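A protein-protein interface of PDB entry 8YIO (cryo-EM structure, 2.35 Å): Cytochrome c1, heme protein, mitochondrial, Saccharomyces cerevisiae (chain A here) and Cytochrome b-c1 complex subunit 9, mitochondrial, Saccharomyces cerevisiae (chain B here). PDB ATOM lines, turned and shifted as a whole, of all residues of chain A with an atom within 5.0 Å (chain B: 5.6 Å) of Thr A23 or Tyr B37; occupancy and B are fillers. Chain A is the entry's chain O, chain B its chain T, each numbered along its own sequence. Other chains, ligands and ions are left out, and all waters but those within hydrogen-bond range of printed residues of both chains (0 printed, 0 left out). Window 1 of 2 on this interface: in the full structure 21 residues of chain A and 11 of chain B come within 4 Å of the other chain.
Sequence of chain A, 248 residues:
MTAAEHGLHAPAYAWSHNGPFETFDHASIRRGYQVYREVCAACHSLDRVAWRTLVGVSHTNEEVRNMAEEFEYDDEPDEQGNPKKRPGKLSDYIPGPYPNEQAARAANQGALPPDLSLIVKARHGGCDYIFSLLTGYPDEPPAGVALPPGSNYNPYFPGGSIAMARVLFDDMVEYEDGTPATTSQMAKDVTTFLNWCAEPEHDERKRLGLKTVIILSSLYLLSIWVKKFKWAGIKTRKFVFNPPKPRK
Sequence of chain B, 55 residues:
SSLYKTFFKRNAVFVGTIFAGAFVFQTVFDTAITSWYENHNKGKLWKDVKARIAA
The backbone carbonyl oxygen (O) of Ser A16 sits at hydrogen-bond distance from the side-chain amino group (NZ) of Lys B44 (3.2 Å).
The side-chain amide nitrogen of Asn B41 lies within hydrogen-bond range of the backbone carbonyl oxygen of Phe A21, 2.9 Å away.
The side-chain carboxylate of Glu A22 sits at hydrogen-bond distance from a ring nitrogen (NE2) of His B40 (3.3 Å).
The side-chain amino group (NZ) of Lys B44 is in salt-bridge range of the side-chain carboxylate (OE1) of Glu A22, at 3.7 Å.
N of Thr A23 is in hydrogen-bond range of OD1 of Asn B41 (3.2 Å).
O of Thr A23 is in hydrogen-bond range of NZ of Lys B44, 3.3 Å away.
O of Asp A203 sits at hydrogen-bond distance from OH of Tyr B37 (3.3 Å).
The guanidinium group (NH2) of Arg A207 is in hydrogen-bond range of the side-chain hydroxyl (OG1) of Thr B34 (3.2 Å).
O of His A17 lies within hydrogen-bond range of NZ of Lys A206 (3.2 Å).
NZ of Lys A206 sits close to O of Glu A22, 3.5 Å away.
The backbone NH of Phe A24 sits at hydrogen-bond distance from the side-chain carboxylate of Asp A203 (3.2 Å).
A ring nitrogen (ND1) of His A202 lies within hydrogen-bond range of the side-chain carboxylate of Asp A203 (2.9 Å).
The backbone carbonyl oxygen of Tyr B37 lies within hydrogen-bond range of the side-chain amide nitrogen of Asn B41, 3.0 Å away.
The side-chain amino group (NZ) of Lys B44 lies within hydrogen-bond range of the side-chain amide oxygen (OD1) of Asn B41, at 3.4 Å.
CE1 of Tyr B37 touches O of Phe A21, at 3.8 Å.
Phe A21 touches His B40 (O to CD2, 3.4 Å).
Glu A22 touches Tyr B37 (O to OH, 3.998 Å).
CA of Glu A22 touches OD1 of Asn B41 (3.5 Å).
CG2 of Thr A23 touches OH of Tyr B37 (3.3 Å).
Phe A24 touches Lys B44.
OH of Tyr B37 touches CB of Lys A206, at 3.6 Å.
Arg A207 touches Tyr B37.
Ile B33 touches Leu A210 (CG2 to CD2, 3.8 Å).
Of the printed residues of chain B, Thr A23 touches Tyr B37, Asn B41 and Lys B44.
Of the printed residues of chain A, Tyr B37 touches Phe A21, Glu A22, Thr A23, Asp A203, Lys A206 and Arg A207.
Of the printed residues of chain A, Thr B34 touches Arg A207.
Of the printed residues of chain A, Asn B41 touches Phe A21, Glu A22 and Thr A23.
Of the printed residues of chain B, Phe A21 touches Tyr B37 (3.8 Å), His B40 (3.4 Å) and Asn B41 (2.9 Å).
Of the printed residues of chain B, Arg A207 touches Thr B34 and Tyr B37.
Of the printed residues of chain B, Ser A16 touches Lys B44.
The nearest residue of chain B that does not touch Thr A23 is Leu B45 (4.1 Å).
The nearest printed residue of chain A that does not touch Thr B34 is Leu A210 (6.8 Å).
Hydrophobic or aromatic side chains of chain B within 4 Å of the printed part of chain A: Ile B33, Tyr B37 and His B40.
Hydrophobic or aromatic side chains of chain A that line the printed part of chain B: Phe A21 and Leu A210.
Among the printed residues, Asp or Glu carboxylates within 4 Å of a Lys or Arg side-chain nitrogen of the other chain: Glu A22 with Lys B44 (3.7 Å).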
ATOM      1  N   SER A  16      -2.282 -16.809 -16.832  1.00  0.00           N
ATOM      2  CA  SER A  16      -3.309 -16.494 -15.847  1.00  0.00           C
ATOM      3  C   SER A  16      -4.017 -17.726 -15.297  1.00  0.00           C
ATOM      4  O   SER A  16      -4.845 -17.584 -14.393  1.00  0.00           O
ATOM      5  CB  SER A  16      -4.334 -15.522 -16.440  1.00  0.00           C
ATOM      6  OG  SER A  16      -5.130 -16.140 -17.432  1.00  0.00           O
ATOM      7  N   HIS A  17      -3.715 -18.920 -15.801  1.00  0.00           N
ATOM      8  CA  HIS A  17      -4.206 -20.155 -15.209  1.00  0.00           C
ATOM      9  C   HIS A  17      -3.148 -20.873 -14.377  1.00  0.00           C
ATOM     10  O   HIS A  17      -3.405 -21.978 -13.896  1.00  0.00           O
ATOM     11  CB  HIS A  17      -4.747 -21.126 -16.272  1.00  0.00           C
ATOM     12  CG  HIS A  17      -3.847 -21.313 -17.455  1.00  0.00           C
ATOM     13  ND1 HIS A  17      -3.874 -20.479 -18.552  1.00  0.00           N
ATOM     14  CD2 HIS A  17      -2.900 -22.244 -17.718  1.00  0.00           C
ATOM     15  CE1 HIS A  17      -2.997 -20.899 -19.445  1.00  0.00           C
ATOM     16  NE2 HIS A  17      -2.391 -21.967 -18.963  1.00  0.00           N
ATOM     17  N   PHE A  21      -5.628 -21.708  -7.525  1.00  0.00           N
ATOM     18  CA  PHE A  21      -6.981 -21.169  -7.441  1.00  0.00           C
ATOM     19  C   PHE A  21      -7.452 -20.516  -8.736  1.00  0.00           C
ATOM     20  O   PHE A  21      -8.456 -19.799  -8.720  1.00  0.00           O
ATOM     21  CB  PHE A  21      -7.081 -20.158  -6.295  1.00  0.00           C
ATOM     22  CG  PHE A  21      -6.585 -20.677  -4.975  1.00  0.00           C
ATOM     23  CD1 PHE A  21      -6.991 -21.913  -4.500  1.00  0.00           C
ATOM     24  CD2 PHE A  21      -5.717 -19.921  -4.205  1.00  0.00           C
ATOM     25  CE1 PHE A  21      -6.532 -22.389  -3.288  1.00  0.00           C
ATOM     26  CE2 PHE A  21      -5.259 -20.392  -2.993  1.00  0.00           C
ATOM     27  CZ  PHE A  21      -5.668 -21.627  -2.533  1.00  0.00           C
ATOM     28  N   GLU A  22      -6.771 -20.746  -9.853  1.00  0.00           N
ATOM     29  CA  GLU A  22      -7.076 -20.054 -11.097  1.00  0.00           C
ATOM     30  C   GLU A  22      -7.801 -20.960 -12.084  1.00  0.00           C
ATOM     31  O   GLU A  22      -7.549 -22.163 -12.154  1.00  0.00           O
ATOM     32  CB  GLU A  22      -5.802 -19.514 -11.747  1.00  0.00           C
ATOM     33  CG  GLU A  22      -4.835 -18.870 -10.781  1.00  0.00           C
ATOM     34  CD  GLU A  22      -5.432 -17.690 -10.047  1.00  0.00           C
ATOM     35  OE1 GLU A  22      -6.134 -16.880 -10.684  1.00  0.00           O
ATOM     36  OE2 GLU A  22      -5.200 -17.571  -8.828  1.00  0.00           O
ATOM     37  N   THR A  23      -8.708 -20.360 -12.850  1.00  0.00           N
ATOM     38  CA  THR A  23      -9.369 -21.021 -13.962  1.00  0.00           C
ATOM     39  C   THR A  23      -8.755 -20.546 -15.277  1.00  0.00           C
ATOM     40  O   THR A  23      -7.854 -19.708 -15.309  1.00  0.00           O
ATOM     41  CB  THR A  23     -10.877 -20.750 -13.947  1.00  0.00           C
ATOM     42  OG1 THR A  23     -11.125 -19.383 -14.296  1.00  0.00           O
ATOM     43  CG2 THR A  23     -11.466 -21.027 -12.587  1.00  0.00           C
ATOM     44  N   PHE A  24      -9.255 -21.094 -16.380  1.00  0.00           N
ATOM     45  CA  PHE A  24      -8.894 -20.588 -17.695  1.00  0.00           C
ATOM     46  C   PHE A  24      -9.533 -19.224 -17.932  1.00  0.00           C
ATOM     47  O   PHE A  24     -10.547 -18.874 -17.327  1.00  0.00           O
ATOM     48  CB  PHE A  24      -9.349 -21.554 -18.792  1.00  0.00           C
ATOM     49  CG  PHE A  24      -8.445 -22.737 -18.990  1.00  0.00           C
ATOM     50  CD1 PHE A  24      -7.077 -22.573 -19.115  1.00  0.00           C
ATOM     51  CD2 PHE A  24      -8.972 -24.014 -19.073  1.00  0.00           C
ATOM     52  CE1 PHE A  24      -6.249 -23.666 -19.303  1.00  0.00           C
ATOM     53  CE2 PHE A  24      -8.153 -25.108 -19.262  1.00  0.00           C
ATOM     54  CZ  PHE A  24      -6.787 -24.932 -19.375  1.00  0.00           C
ATOM     55  N   ASP A  25      -8.922 -18.447 -18.819  1.00  0.00           N
ATOM     56  CA  ASP A  25      -9.532 -17.231 -19.344  1.00  0.00           C
ATOM     57  C   ASP A  25     -10.342 -17.626 -20.574  1.00  0.00           C
ATOM     58  O   ASP A  25      -9.774 -17.958 -21.618  1.00  0.00           O
ATOM     59  CB  ASP A  25      -8.465 -16.193 -19.681  1.00  0.00           C
ATOM     60  CG  ASP A  25      -9.050 -14.856 -20.101  1.00  0.00           C
ATOM     61  OD1 ASP A  25     -10.252 -14.615 -19.875  1.00  0.00           O
ATOM     62  OD2 ASP A  25      -8.299 -14.035 -20.661  1.00  0.00           O
ATOM     63  N   HIS A 202      -9.941 -29.110 -16.289  1.00  0.00           N
ATOM     64  CA  HIS A 202      -9.014 -28.285 -15.512  1.00  0.00           C
ATOM     65  C   HIS A 202      -9.719 -27.399 -14.485  1.00  0.00           C
ATOM     66  O   HIS A 202      -9.282 -27.302 -13.334  1.00  0.00           O
ATOM     67  CB  HIS A 202      -8.187 -27.443 -16.491  1.00  0.00           C
ATOM     68  CG  HIS A 202      -7.337 -26.389 -15.853  1.00  0.00           C
ATOM     69  ND1 HIS A 202      -7.798 -25.118 -15.584  1.00  0.00           N
ATOM     70  CD2 HIS A 202      -6.035 -26.400 -15.481  1.00  0.00           C
ATOM     71  CE1 HIS A 202      -6.827 -24.402 -15.049  1.00  0.00           C
ATOM     72  NE2 HIS A 202      -5.747 -25.157 -14.977  1.00  0.00           N
ATOM     73  N   ASP A 203     -10.818 -26.752 -14.882  1.00  0.00           N
ATOM     74  CA  ASP A 203     -11.522 -25.865 -13.960  1.00  0.00           C
ATOM     75  C   ASP A 203     -12.282 -26.640 -12.893  1.00  0.00           C
ATOM     76  O   ASP A 203     -12.420 -26.163 -11.765  1.00  0.00           O
ATOM     77  CB  ASP A 203     -12.475 -24.951 -14.729  1.00  0.00           C
ATOM     78  CG  ASP A 203     -11.747 -23.919 -15.563  1.00  0.00           C
ATOM     79  OD1 ASP A 203     -10.504 -23.961 -15.610  1.00  0.00           O
ATOM     80  OD2 ASP A 203     -12.415 -23.061 -16.170  1.00  0.00           O
ATOM     81  N   LYS A 206      -9.658 -28.313 -10.097  1.00  0.00           N
ATOM     82  CA  LYS A 206      -9.139 -27.420  -9.071  1.00  0.00           C
ATOM     83  C   LYS A 206     -10.200 -27.030  -8.049  1.00  0.00           C
ATOM     84  O   LYS A 206      -9.858 -26.721  -6.904  1.00  0.00           O
ATOM     85  CB  LYS A 206      -8.538 -26.179  -9.722  1.00  0.00           C
ATOM     86  CG  LYS A 206      -7.183 -26.432 -10.347  1.00  0.00           C
ATOM     87  CD  LYS A 206      -6.637 -25.179 -10.982  1.00  0.00           C
ATOM     88  CE  LYS A 206      -5.174 -25.320 -11.309  1.00  0.00           C
ATOM     89  NZ  LYS A 206      -4.635 -24.065 -11.879  1.00  0.00           N
ATOM     90  N   ARG A 207     -11.478 -27.045  -8.428  1.00  0.00           N
ATOM     91  CA  ARG A 207     -12.536 -26.779  -7.460  1.00  0.00           C
ATOM     92  C   ARG A 207     -12.768 -27.974  -6.543  1.00  0.00           C
ATOM     93  O   ARG A 207     -13.008 -27.800  -5.345  1.00  0.00           O
ATOM     94  CB  ARG A 207     -13.830 -26.397  -8.179  1.00  0.00           C
ATOM     95  CG  ARG A 207     -14.890 -25.813  -7.260  1.00  0.00           C
ATOM     96  CD  ARG A 207     -16.230 -25.627  -7.957  1.00  0.00           C
ATOM     97  NE  ARG A 207     -16.797 -26.888  -8.424  1.00  0.00           N
ATOM     98  CZ  ARG A 207     -17.552 -27.692  -7.685  1.00  0.00           C
ATOM     99  NH1 ARG A 207     -18.021 -28.819  -8.198  1.00  0.00           N
ATOM    100  NH2 ARG A 207     -17.838 -27.374  -6.432  1.00  0.00           N
ATOM    101  N   LEU A 210      -9.960 -28.287  -3.829  1.00  0.00           N
ATOM    102  CA  LEU A 210     -10.007 -27.374  -2.691  1.00  0.00           C
ATOM    103  C   LEU A 210     -10.873 -27.932  -1.566  1.00  0.00           C
ATOM    104  O   LEU A 210     -10.560 -27.744  -0.388  1.00  0.00           O
ATOM    105  CB  LEU A 210     -10.517 -26.006  -3.143  1.00  0.00           C
ATOM    106  CG  LEU A 210     -10.567 -24.874  -2.117  1.00  0.00           C
ATOM    107  CD1 LEU A 210      -9.191 -24.599  -1.546  1.00  0.00           C
ATOM    108  CD2 LEU A 210     -11.149 -23.619  -2.742  1.00  0.00           C
ATOM    109  N   ALA B  32     -20.466 -22.752  -0.040  1.00  0.00           N
ATOM    110  CA  ALA B  32     -19.538 -21.718   0.407  1.00  0.00           C
ATOM    111  C   ALA B  32     -18.268 -21.690  -0.436  1.00  0.00           C
ATOM    112  O   ALA B  32     -17.731 -20.614  -0.717  1.00  0.00           O
ATOM    113  CB  ALA B  32     -19.196 -21.931   1.881  1.00  0.00           C
ATOM    114  N   ILE B  33     -17.774 -22.858  -0.851  1.00  0.00           N
ATOM    115  CA  ILE B  33     -16.529 -22.912  -1.611  1.00  0.00           C
ATOM    116  C   ILE B  33     -16.749 -22.465  -3.052  1.00  0.00           C
ATOM    117  O   ILE B  33     -15.935 -21.713  -3.605  1.00  0.00           O
ATOM    118  CB  ILE B  33     -15.926 -24.327  -1.524  1.00  0.00           C
ATOM    119  CG1 ILE B  33     -15.354 -24.553  -0.127  1.00  0.00           C
ATOM    120  CG2 ILE B  33     -14.858 -24.560  -2.593  1.00  0.00           C
ATOM    121  CD1 ILE B  33     -14.594 -25.828   0.012  1.00  0.00           C
ATOM    122  N   THR B  34     -17.862 -22.894  -3.661  1.00  0.00           N
ATOM    123  CA  THR B  34     -18.173 -22.532  -5.043  1.00  0.00           C
ATOM    124  C   THR B  34     -18.372 -21.026  -5.192  1.00  0.00           C
ATOM    125  O   THR B  34     -17.940 -20.429  -6.185  1.00  0.00           O
ATOM    126  CB  THR B  34     -19.418 -23.299  -5.505  1.00  0.00           C
ATOM    127  OG1 THR B  34     -19.184 -24.707  -5.386  1.00  0.00           O
ATOM    128  CG2 THR B  34     -19.763 -22.993  -6.954  1.00  0.00           C
ATOM    129  N   SER B  35     -18.970 -20.388  -4.182  1.00  0.00           N
ATOM    130  CA  SER B  35     -19.146 -18.940  -4.217  1.00  0.00           C
ATOM    131  C   SER B  35     -17.818 -18.211  -4.054  1.00  0.00           C
ATOM    132  O   SER B  35     -17.608 -17.156  -4.662  1.00  0.00           O
ATOM    133  CB  SER B  35     -20.129 -18.510  -3.130  1.00  0.00           C
ATOM    134  OG  SER B  35     -20.087 -17.110  -2.933  1.00  0.00           O
ATOM    135  N   TRP B  36     -16.911 -18.757  -3.239  1.00  0.00           N
ATOM    136  CA  TRP B  36     -15.588 -18.156  -3.096  1.00  0.00           C
ATOM    137  C   TRP B  36     -14.744 -18.375  -4.345  1.00  0.00           C
ATOM    138  O   TRP B  36     -13.983 -17.488  -4.748  1.00  0.00           O
ATOM    139  CB  TRP B  36     -14.874 -18.727  -1.868  1.00  0.00           C
ATOM    140  CG  TRP B  36     -13.527 -18.101  -1.619  1.00  0.00           C
ATOM    141  CD1 TRP B  36     -13.267 -17.001  -0.860  1.00  0.00           C
ATOM    142  CD2 TRP B  36     -12.261 -18.531  -2.142  1.00  0.00           C
ATOM    143  NE1 TRP B  36     -11.926 -16.717  -0.877  1.00  0.00           N
ATOM    144  CE2 TRP B  36     -11.286 -17.642  -1.657  1.00  0.00           C
ATOM    145  CE3 TRP B  36     -11.860 -19.581  -2.977  1.00  0.00           C
ATOM    146  CZ2 TRP B  36      -9.937 -17.769  -1.976  1.00  0.00           C
ATOM    147  CZ3 TRP B  36     -10.521 -19.703  -3.292  1.00  0.00           C
ATOM    148  CH2 TRP B  36      -9.576 -18.804  -2.793  1.00  0.00           C
ATOM    149  N   TYR B  37     -14.857 -19.556  -4.957  1.00  0.00           N
ATOM    150  CA  TYR B  37     -14.032 -19.909  -6.107  1.00  0.00           C
ATOM    151  C   TYR B  37     -14.421 -19.115  -7.346  1.00  0.00           C
ATOM    152  O   TYR B  37     -13.553 -18.764  -8.152  1.00  0.00           O
ATOM    153  CB  TYR B  37     -14.144 -21.413  -6.366  1.00  0.00           C
ATOM    154  CG  TYR B  37     -13.276 -21.970  -7.475  1.00  0.00           C
ATOM    155  CD1 TYR B  37     -11.894 -22.031  -7.341  1.00  0.00           C
ATOM    156  CD2 TYR B  37     -13.846 -22.469  -8.641  1.00  0.00           C
ATOM    157  CE1 TYR B  37     -11.103 -22.555  -8.344  1.00  0.00           C
ATOM    158  CE2 TYR B  37     -13.063 -22.997  -9.650  1.00  0.00           C
ATOM    159  CZ  TYR B  37     -11.693 -23.038  -9.495  1.00  0.00           C
ATOM    160  OH  TYR B  37     -10.908 -23.558 -10.494  1.00  0.00           O
ATOM    161  N   GLU B  38     -15.708 -18.809  -7.506  1.00  0.00           N
ATOM    162  CA  GLU B  38     -16.155 -18.051  -8.668  1.00  0.00           C
ATOM    163  C   GLU B  38     -15.929 -16.555  -8.506  1.00  0.00           C
ATOM    164  O   GLU B  38     -15.740 -15.854  -9.505  1.00  0.00           O
ATOM    165  CB  GLU B  38     -17.631 -18.334  -8.947  1.00  0.00           C
ATOM    166  CG  GLU B  38     -17.895 -19.751  -9.419  1.00  0.00           C
ATOM    167  CD  GLU B  38     -19.363 -20.022  -9.671  1.00  0.00           C
ATOM    168  OE1 GLU B  38     -20.193 -19.141  -9.368  1.00  0.00           O
ATOM    169  OE2 GLU B  38     -19.687 -21.116 -10.174  1.00  0.00           O
ATOM    170  N   ASN B  39     -15.949 -16.047  -7.273  1.00  0.00           N
ATOM    171  CA  ASN B  39     -15.664 -14.633  -7.055  1.00  0.00           C
ATOM    172  C   ASN B  39     -14.181 -14.323  -7.201  1.00  0.00           C
ATOM    173  O   ASN B  39     -13.821 -13.211  -7.600  1.00  0.00           O
ATOM    174  CB  ASN B  39     -16.155 -14.203  -5.673  1.00  0.00           C
ATOM    175  CG  ASN B  39     -16.179 -12.702  -5.510  1.00  0.00           C
ATOM    176  OD1 ASN B  39     -15.290 -12.119  -4.892  1.00  0.00           O
ATOM    177  ND2 ASN B  39     -17.195 -12.063  -6.074  1.00  0.00           N
ATOM    178  N   HIS B  40     -13.319 -15.290  -6.884  1.00  0.00           N
ATOM    179  CA  HIS B  40     -11.883 -15.120  -7.078  1.00  0.00           C
ATOM    180  C   HIS B  40     -11.519 -15.086  -8.558  1.00  0.00           C
ATOM    181  O   HIS B  40     -10.508 -14.483  -8.933  1.00  0.00           O
ATOM    182  CB  HIS B  40     -11.140 -16.249  -6.359  1.00  0.00           C
ATOM    183  CG  HIS B  40      -9.649 -16.151  -6.439  1.00  0.00           C
ATOM    184  ND1 HIS B  40      -8.904 -15.388  -5.567  1.00  0.00           N
ATOM    185  CD2 HIS B  40      -8.763 -16.731  -7.281  1.00  0.00           C
ATOM    186  CE1 HIS B  40      -7.624 -15.497  -5.872  1.00  0.00           C
ATOM    187  NE2 HIS B  40      -7.511 -16.306  -6.909  1.00  0.00           N
ATOM    188  N   ASN B  41     -12.337 -15.703  -9.410  1.00  0.00           N
ATOM    189  CA  ASN B  41     -12.080 -15.793 -10.841  1.00  0.00           C
ATOM    190  C   ASN B  41     -13.122 -15.039 -11.661  1.00  0.00           C
ATOM    191  O   ASN B  41     -13.493 -15.481 -12.751  1.00  0.00           O
ATOM    192  CB  ASN B  41     -11.995 -17.248 -11.295  1.00  0.00           C
ATOM    193  CG  ASN B  41     -10.788 -17.965 -10.733  1.00  0.00           C
ATOM    194  OD1 ASN B  41      -9.665 -17.756 -11.181  1.00  0.00           O
ATOM    195  ND2 ASN B  41     -11.017 -18.818  -9.747  1.00  0.00           N
ATOM    196  N   LYS B  44     -13.513 -13.996 -15.858  1.00  0.00           N
ATOM    197  CA  LYS B  44     -12.873 -15.020 -16.668  1.00  0.00           C
ATOM    198  C   LYS B  44     -13.782 -16.180 -17.033  1.00  0.00           C
ATOM    199  O   LYS B  44     -13.443 -16.935 -17.947  1.00  0.00           O
ATOM    200  CB  LYS B  44     -11.636 -15.586 -15.950  1.00  0.00           C
ATOM    201  CG  LYS B  44     -10.489 -14.606 -15.806  1.00  0.00           C
ATOM    202  CD  LYS B  44      -9.179 -15.327 -15.535  1.00  0.00           C
ATOM    203  CE  LYS B  44      -9.233 -16.099 -14.231  1.00  0.00           C
ATOM    204  NZ  LYS B  44      -7.921 -16.699 -13.884  1.00  0.00           N
ATOM    205  N   LEU B  45     -14.915 -16.344 -16.356  1.00  0.00           N
ATOM    206  CA  LEU B  45     -15.808 -17.459 -16.615  1.00  0.00           C
ATOM    207  C   LEU B  45     -16.614 -17.216 -17.887  1.00  0.00           C
ATOM    208  O   LEU B  45     -16.645 -16.111 -18.435  1.00  0.00           O
ATOM    209  CB  LEU B  45     -16.738 -17.683 -15.427  1.00  0.00           C
ATOM    210  CG  LEU B  45     -16.056 -17.793 -14.064  1.00  0.00           C
ATOM    211  CD1 LEU B  45     -17.084 -17.782 -12.950  1.00  0.00           C
ATOM    212  CD2 LEU B  45     -15.200 -19.043 -13.990  1.00  0.00           C
